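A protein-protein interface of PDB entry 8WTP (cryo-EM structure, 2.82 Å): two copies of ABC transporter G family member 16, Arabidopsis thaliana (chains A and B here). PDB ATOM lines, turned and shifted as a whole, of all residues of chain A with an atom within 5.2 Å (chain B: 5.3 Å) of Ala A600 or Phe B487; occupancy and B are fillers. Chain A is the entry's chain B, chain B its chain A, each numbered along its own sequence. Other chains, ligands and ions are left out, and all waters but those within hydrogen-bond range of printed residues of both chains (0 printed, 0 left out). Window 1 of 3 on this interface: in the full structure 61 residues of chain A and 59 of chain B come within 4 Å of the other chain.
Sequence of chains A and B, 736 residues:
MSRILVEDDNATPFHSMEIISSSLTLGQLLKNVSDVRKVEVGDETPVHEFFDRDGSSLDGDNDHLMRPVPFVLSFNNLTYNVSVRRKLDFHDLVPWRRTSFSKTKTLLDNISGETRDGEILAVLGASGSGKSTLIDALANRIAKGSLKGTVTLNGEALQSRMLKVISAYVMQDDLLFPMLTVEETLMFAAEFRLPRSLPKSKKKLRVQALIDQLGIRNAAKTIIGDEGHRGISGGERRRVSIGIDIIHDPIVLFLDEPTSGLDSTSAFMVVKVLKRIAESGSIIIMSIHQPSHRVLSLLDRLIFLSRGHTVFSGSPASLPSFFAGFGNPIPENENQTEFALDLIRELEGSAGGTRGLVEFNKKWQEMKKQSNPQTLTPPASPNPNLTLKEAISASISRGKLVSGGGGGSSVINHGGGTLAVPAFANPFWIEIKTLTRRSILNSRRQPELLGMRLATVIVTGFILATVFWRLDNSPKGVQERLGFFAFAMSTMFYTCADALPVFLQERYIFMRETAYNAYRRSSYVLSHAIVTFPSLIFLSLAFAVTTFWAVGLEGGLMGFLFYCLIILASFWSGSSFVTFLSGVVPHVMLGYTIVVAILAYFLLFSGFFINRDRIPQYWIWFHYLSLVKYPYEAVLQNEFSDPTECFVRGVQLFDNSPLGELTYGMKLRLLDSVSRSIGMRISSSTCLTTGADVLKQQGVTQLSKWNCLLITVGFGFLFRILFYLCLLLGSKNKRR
Of the 12 printed residues of chain B, 4 touch a printed residue of chain A.
Hydrophobic or aromatic side chains of chain B within 4 Å of the printed part of chain A: Leu B464 and Phe B487.
Hydrophobic or aromatic side chains of chain A that line the printed part of chain B: Ala A600, Tyr A601, Leu A604 and Phe A609.
The side-chain hydroxyl of Thr B491 sits at hydrogen-bond distance from the backbone carbonyl oxygen of Phe B487, 2.8 Å away.
OH of Tyr A601 is in hydrogen-bond range of OG1 of Thr B460, 2.5 Å away.
Ala A600 touches just one residue of chain B: Phe B487.
Of the printed residues of chain B, Phe A609 touches Gly B483 (3.1 Å).
Printed residues of chain B within 4 Å of Leu A604: Leu B464 and Phe B487.
Phe B484 touches none of the printed residues of chain A.
The nearest printed residue of chain A that does not touch Phe B487 is Phe A609 (4.05 Å).
No position is printed for both chains.
Of the 5 pairs that touch across the chains among the printed residues, none has its exchanged pair printed and touching as well.
Among the printed residues, pairs that only touch across the chains: Ala A600 with Phe B487 (3.2 Å), Leu A604 with Leu B464 (3.9 Å), Leu A604 with Phe B487 (3.9 Å) and Phe A609 with Gly B483 (3.1 Å).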
ATOM      1  N   VAL A 595     -17.419   8.781   5.669  1.00  0.00           N
ATOM      2  CA  VAL A 595     -17.115  10.064   6.282  1.00  0.00           C
ATOM      3  C   VAL A 595     -16.578  11.035   5.247  1.00  0.00           C
ATOM      4  O   VAL A 595     -16.985  12.194   5.198  1.00  0.00           O
ATOM      5  CB  VAL A 595     -16.135   9.870   7.458  1.00  0.00           C
ATOM      6  CG1 VAL A 595     -15.600  11.177   7.931  1.00  0.00           C
ATOM      7  CG2 VAL A 595     -16.838   9.207   8.596  1.00  0.00           C
ATOM      8  N   VAL A 596     -15.697  10.563   4.368  1.00  0.00           N
ATOM      9  CA  VAL A 596     -15.225  11.378   3.257  1.00  0.00           C
ATOM     10  C   VAL A 596     -16.348  11.643   2.261  1.00  0.00           C
ATOM     11  O   VAL A 596     -16.402  12.712   1.650  1.00  0.00           O
ATOM     12  CB  VAL A 596     -14.015  10.685   2.611  1.00  0.00           C
ATOM     13  CG1 VAL A 596     -13.437  11.496   1.482  1.00  0.00           C
ATOM     14  CG2 VAL A 596     -12.963  10.478   3.639  1.00  0.00           C
ATOM     15  N   ALA A 597     -17.290  10.716   2.116  1.00  0.00           N
ATOM     16  CA  ALA A 597     -18.357  10.910   1.143  1.00  0.00           C
ATOM     17  C   ALA A 597     -19.395  11.901   1.637  1.00  0.00           C
ATOM     18  O   ALA A 597     -19.959  12.648   0.839  1.00  0.00           O
ATOM     19  CB  ALA A 597     -19.018   9.580   0.812  1.00  0.00           C
ATOM     20  N   ILE A 598     -19.671  11.928   2.936  1.00  0.00           N
ATOM     21  CA  ILE A 598     -20.658  12.870   3.449  1.00  0.00           C
ATOM     22  C   ILE A 598     -20.054  14.257   3.592  1.00  0.00           C
ATOM     23  O   ILE A 598     -20.679  15.256   3.228  1.00  0.00           O
ATOM     24  CB  ILE A 598     -21.254  12.354   4.768  1.00  0.00           C
ATOM     25  CG1 ILE A 598     -22.105  11.123   4.495  1.00  0.00           C
ATOM     26  CG2 ILE A 598     -22.159  13.362   5.380  1.00  0.00           C
ATOM     27  CD1 ILE A 598     -22.634  10.453   5.735  1.00  0.00           C
ATOM     28  N   LEU A 599     -18.814  14.353   4.053  1.00  0.00           N
ATOM     29  CA  LEU A 599     -18.170  15.653   4.178  1.00  0.00           C
ATOM     30  C   LEU A 599     -17.709  16.229   2.851  1.00  0.00           C
ATOM     31  O   LEU A 599     -17.170  17.335   2.839  1.00  0.00           O
ATOM     32  CB  LEU A 599     -16.983  15.573   5.129  1.00  0.00           C
ATOM     33  CG  LEU A 599     -17.271  15.107   6.553  1.00  0.00           C
ATOM     34  CD1 LEU A 599     -15.973  14.775   7.199  1.00  0.00           C
ATOM     35  CD2 LEU A 599     -18.035  16.118   7.384  1.00  0.00           C
ATOM     36  N   ALA A 600     -17.872  15.508   1.748  1.00  0.00           N
ATOM     37  CA  ALA A 600     -17.750  16.084   0.422  1.00  0.00           C
ATOM     38  C   ALA A 600     -19.083  16.557  -0.115  1.00  0.00           C
ATOM     39  O   ALA A 600     -19.123  17.518  -0.880  1.00  0.00           O
ATOM     40  CB  ALA A 600     -17.149  15.071  -0.544  1.00  0.00           C
ATOM     41  N   TYR A 601     -20.182  15.909   0.269  1.00  0.00           N
ATOM     42  CA  TYR A 601     -21.503  16.422  -0.063  1.00  0.00           C
ATOM     43  C   TYR A 601     -21.933  17.534   0.871  1.00  0.00           C
ATOM     44  O   TYR A 601     -22.859  18.271   0.547  1.00  0.00           O
ATOM     45  CB  TYR A 601     -22.555  15.320  -0.018  1.00  0.00           C
ATOM     46  CG  TYR A 601     -22.298  14.173  -0.951  1.00  0.00           C
ATOM     47  CD1 TYR A 601     -21.644  14.359  -2.154  1.00  0.00           C
ATOM     48  CD2 TYR A 601     -22.731  12.903  -0.635  1.00  0.00           C
ATOM     49  CE1 TYR A 601     -21.407  13.316  -2.994  1.00  0.00           C
ATOM     50  CE2 TYR A 601     -22.499  11.853  -1.472  1.00  0.00           C
ATOM     51  CZ  TYR A 601     -21.838  12.066  -2.648  1.00  0.00           C
ATOM     52  OH  TYR A 601     -21.613  11.007  -3.481  1.00  0.00           O
ATOM     53  N   PHE A 602     -21.306  17.653   2.035  1.00  0.00           N
ATOM     54  CA  PHE A 602     -21.520  18.827   2.859  1.00  0.00           C
ATOM     55  C   PHE A 602     -20.841  20.043   2.263  1.00  0.00           C
ATOM     56  O   PHE A 602     -21.338  21.159   2.415  1.00  0.00           O
ATOM     57  CB  PHE A 602     -20.993  18.581   4.264  1.00  0.00           C
ATOM     58  CG  PHE A 602     -21.920  17.811   5.141  1.00  0.00           C
ATOM     59  CD1 PHE A 602     -23.247  17.639   4.801  1.00  0.00           C
ATOM     60  CD2 PHE A 602     -21.461  17.261   6.315  1.00  0.00           C
ATOM     61  CE1 PHE A 602     -24.086  16.935   5.608  1.00  0.00           C
ATOM     62  CE2 PHE A 602     -22.296  16.552   7.113  1.00  0.00           C
ATOM     63  CZ  PHE A 602     -23.613  16.397   6.766  1.00  0.00           C
ATOM     64  N   LEU A 603     -19.704  19.845   1.598  1.00  0.00           N
ATOM     65  CA  LEU A 603     -18.955  20.922   0.967  1.00  0.00           C
ATOM     66  C   LEU A 603     -19.586  21.363  -0.343  1.00  0.00           C
ATOM     67  O   LEU A 603     -19.560  22.553  -0.665  1.00  0.00           O
ATOM     68  CB  LEU A 603     -17.515  20.472   0.737  1.00  0.00           C
ATOM     69  CG  LEU A 603     -16.594  21.272  -0.174  1.00  0.00           C
ATOM     70  CD1 LEU A 603     -16.227  22.582   0.450  1.00  0.00           C
ATOM     71  CD2 LEU A 603     -15.359  20.480  -0.507  1.00  0.00           C
ATOM     72  N   LEU A 604     -20.157  20.424  -1.095  1.00  0.00           N
ATOM     73  CA  LEU A 604     -20.888  20.751  -2.312  1.00  0.00           C
ATOM     74  C   LEU A 604     -22.110  21.611  -2.025  1.00  0.00           C
ATOM     75  O   LEU A 604     -22.459  22.484  -2.824  1.00  0.00           O
ATOM     76  CB  LEU A 604     -21.294  19.459  -3.009  1.00  0.00           C
ATOM     77  CG  LEU A 604     -22.160  19.492  -4.257  1.00  0.00           C
ATOM     78  CD1 LEU A 604     -21.402  20.136  -5.369  1.00  0.00           C
ATOM     79  CD2 LEU A 604     -22.555  18.096  -4.637  1.00  0.00           C
ATOM     80  N   PHE A 609     -19.802  25.753  -4.207  1.00  0.00           N
ATOM     81  CA  PHE A 609     -19.856  25.211  -5.558  1.00  0.00           C
ATOM     82  C   PHE A 609     -21.082  25.716  -6.306  1.00  0.00           C
ATOM     83  O   PHE A 609     -20.987  26.093  -7.476  1.00  0.00           O
ATOM     84  CB  PHE A 609     -19.857  23.688  -5.508  1.00  0.00           C
ATOM     85  CG  PHE A 609     -18.527  23.088  -5.203  1.00  0.00           C
ATOM     86  CD1 PHE A 609     -18.067  23.002  -3.913  1.00  0.00           C
ATOM     87  CD2 PHE A 609     -17.740  22.597  -6.209  1.00  0.00           C
ATOM     88  CE1 PHE A 609     -16.853  22.446  -3.642  1.00  0.00           C
ATOM     89  CE2 PHE A 609     -16.521  22.034  -5.937  1.00  0.00           C
ATOM     90  CZ  PHE A 609     -16.082  21.961  -4.655  1.00  0.00           C
ATOM     91  N   THR B 460     -23.314   9.531  -6.608  1.00  0.00           N
ATOM     92  CA  THR B 460     -22.737  10.848  -6.857  1.00  0.00           C
ATOM     93  C   THR B 460     -23.146  11.379  -8.220  1.00  0.00           C
ATOM     94  O   THR B 460     -23.270  12.589  -8.401  1.00  0.00           O
ATOM     95  CB  THR B 460     -21.220  10.782  -6.749  1.00  0.00           C
ATOM     96  OG1 THR B 460     -20.870  10.015  -5.596  1.00  0.00           O
ATOM     97  CG2 THR B 460     -20.633  12.155  -6.578  1.00  0.00           C
ATOM     98  N   LEU B 464     -25.049  14.923  -8.346  1.00  0.00           N
ATOM     99  CA  LEU B 464     -24.469  16.004  -9.137  1.00  0.00           C
ATOM    100  C   LEU B 464     -25.337  16.398 -10.318  1.00  0.00           C
ATOM    101  O   LEU B 464     -25.273  17.541 -10.768  1.00  0.00           O
ATOM    102  CB  LEU B 464     -23.091  15.608  -9.648  1.00  0.00           C
ATOM    103  CG  LEU B 464     -21.898  15.710  -8.716  1.00  0.00           C
ATOM    104  CD1 LEU B 464     -20.696  15.204  -9.430  1.00  0.00           C
ATOM    105  CD2 LEU B 464     -21.689  17.125  -8.308  1.00  0.00           C
ATOM    106  N   LEU B 482     -17.771  25.164 -13.613  1.00  0.00           N
ATOM    107  CA  LEU B 482     -16.444  24.907 -13.073  1.00  0.00           C
ATOM    108  C   LEU B 482     -16.517  24.203 -11.731  1.00  0.00           C
ATOM    109  O   LEU B 482     -15.621  23.434 -11.387  1.00  0.00           O
ATOM    110  CB  LEU B 482     -15.667  26.207 -12.925  1.00  0.00           C
ATOM    111  CG  LEU B 482     -15.869  27.333 -13.919  1.00  0.00           C
ATOM    112  CD1 LEU B 482     -15.091  28.502 -13.453  1.00  0.00           C
ATOM    113  CD2 LEU B 482     -15.390  26.947 -15.255  1.00  0.00           C
ATOM    114  N   GLY B 483     -17.573  24.451 -10.961  1.00  0.00           N
ATOM    115  CA  GLY B 483     -17.766  23.722  -9.726  1.00  0.00           C
ATOM    116  C   GLY B 483     -18.326  22.339  -9.930  1.00  0.00           C
ATOM    117  O   GLY B 483     -18.083  21.452  -9.116  1.00  0.00           O
ATOM    118  N   PHE B 484     -19.087  22.130 -10.997  1.00  0.00           N
ATOM    119  CA  PHE B 484     -19.493  20.774 -11.333  1.00  0.00           C
ATOM    120  C   PHE B 484     -18.313  19.967 -11.839  1.00  0.00           C
ATOM    121  O   PHE B 484     -18.105  18.837 -11.402  1.00  0.00           O
ATOM    122  CB  PHE B 484     -20.608  20.786 -12.372  1.00  0.00           C
ATOM    123  CG  PHE B 484     -20.854  19.456 -12.983  1.00  0.00           C
ATOM    124  CD1 PHE B 484     -21.391  18.437 -12.242  1.00  0.00           C
ATOM    125  CD2 PHE B 484     -20.531  19.213 -14.294  1.00  0.00           C
ATOM    126  CE1 PHE B 484     -21.604  17.210 -12.797  1.00  0.00           C
ATOM    127  CE2 PHE B 484     -20.737  17.982 -14.843  1.00  0.00           C
ATOM    128  CZ  PHE B 484     -21.275  16.988 -14.094  1.00  0.00           C
ATOM    129  N   PHE B 485     -17.521  20.536 -12.749  1.00  0.00           N
ATOM    130  CA  PHE B 485     -16.409  19.827 -13.360  1.00  0.00           C
ATOM    131  C   PHE B 485     -15.272  19.567 -12.395  1.00  0.00           C
ATOM    132  O   PHE B 485     -14.461  18.686 -12.657  1.00  0.00           O
ATOM    133  CB  PHE B 485     -15.878  20.606 -14.551  1.00  0.00           C
ATOM    134  CG  PHE B 485     -16.781  20.585 -15.737  1.00  0.00           C
ATOM    135  CD1 PHE B 485     -17.425  19.429 -16.106  1.00  0.00           C
ATOM    136  CD2 PHE B 485     -16.972  21.718 -16.494  1.00  0.00           C
ATOM    137  CE1 PHE B 485     -18.242  19.415 -17.188  1.00  0.00           C
ATOM    138  CE2 PHE B 485     -17.793  21.706 -17.569  1.00  0.00           C
ATOM    139  CZ  PHE B 485     -18.422  20.556 -17.920  1.00  0.00           C
ATOM    140  N   ALA B 486     -15.171  20.309 -11.301  1.00  0.00           N
ATOM    141  CA  ALA B 486     -14.127  20.030 -10.332  1.00  0.00           C
ATOM    142  C   ALA B 486     -14.565  19.024  -9.290  1.00  0.00           C
ATOM    143  O   ALA B 486     -13.728  18.310  -8.740  1.00  0.00           O
ATOM    144  CB  ALA B 486     -13.684  21.312  -9.641  1.00  0.00           C
ATOM    145  N   PHE B 487     -15.858  18.959  -9.000  1.00  0.00           N
ATOM    146  CA  PHE B 487     -16.381  17.923  -8.128  1.00  0.00           C
ATOM    147  C   PHE B 487     -16.587  16.620  -8.874  1.00  0.00           C
ATOM    148  O   PHE B 487     -16.456  15.550  -8.278  1.00  0.00           O
ATOM    149  CB  PHE B 487     -17.699  18.374  -7.503  1.00  0.00           C
ATOM    150  CG  PHE B 487     -18.020  17.687  -6.214  1.00  0.00           C
ATOM    151  CD1 PHE B 487     -17.657  18.251  -5.016  1.00  0.00           C
ATOM    152  CD2 PHE B 487     -18.677  16.470  -6.203  1.00  0.00           C
ATOM    153  CE1 PHE B 487     -17.946  17.621  -3.845  1.00  0.00           C
ATOM    154  CE2 PHE B 487     -18.958  15.838  -5.033  1.00  0.00           C
ATOM    155  CZ  PHE B 487     -18.596  16.413  -3.858  1.00  0.00           C
ATOM    156  N   ALA B 488     -16.937  16.682 -10.158  1.00  0.00           N
ATOM    157  CA  ALA B 488     -17.052  15.465 -10.948  1.00  0.00           C
ATOM    158  C   ALA B 488     -15.692  14.823 -11.141  1.00  0.00           C
ATOM    159  O   ALA B 488     -15.503  13.657 -10.808  1.00  0.00           O
ATOM    160  CB  ALA B 488     -17.703  15.757 -12.294  1.00  0.00           C
ATOM    161  N   MET B 489     -14.708  15.584 -11.600  1.00  0.00           N
ATOM    162  CA  MET B 489     -13.399  15.023 -11.905  1.00  0.00           C
ATOM    163  C   MET B 489     -12.569  14.692 -10.680  1.00  0.00           C
ATOM    164  O   MET B 489     -11.444  14.232 -10.849  1.00  0.00           O
ATOM    165  CB  MET B 489     -12.615  15.974 -12.798  1.00  0.00           C
ATOM    166  CG  MET B 489     -13.191  16.092 -14.176  1.00  0.00           C
ATOM    167  SD  MET B 489     -13.233  14.543 -15.069  1.00  0.00           S
ATOM    168  CE  MET B 489     -14.904  14.604 -15.651  1.00  0.00           C
ATOM    169  N   SER B 490     -13.064  14.931  -9.472  1.00  0.00           N
ATOM    170  CA  SER B 490     -12.437  14.436  -8.261  1.00  0.00           C
ATOM    171  C   SER B 490     -13.106  13.182  -7.736  1.00  0.00           C
ATOM    172  O   SER B 490     -12.524  12.497  -6.894  1.00  0.00           O
ATOM    173  CB  SER B 490     -12.475  15.504  -7.173  1.00  0.00           C
ATOM    174  OG  SER B 490     -11.888  16.695  -7.626  1.00  0.00           O
ATOM    175  N   THR B 491     -14.326  12.894  -8.192  1.00  0.00           N
ATOM    176  CA  THR B 491     -14.990  11.637  -7.881  1.00  0.00           C
ATOM    177  C   THR B 491     -14.243  10.463  -8.483  1.00  0.00           C
ATOM    178  O   THR B 491     -14.209   9.383  -7.892  1.00  0.00           O
ATOM    179  CB  THR B 491     -16.430  11.688  -8.397  1.00  0.00           C
ATOM    180  OG1 THR B 491     -17.062  12.868  -7.903  1.00  0.00           O
ATOM    181  CG2 THR B 491     -17.236  10.493  -7.970  1.00  0.00           C
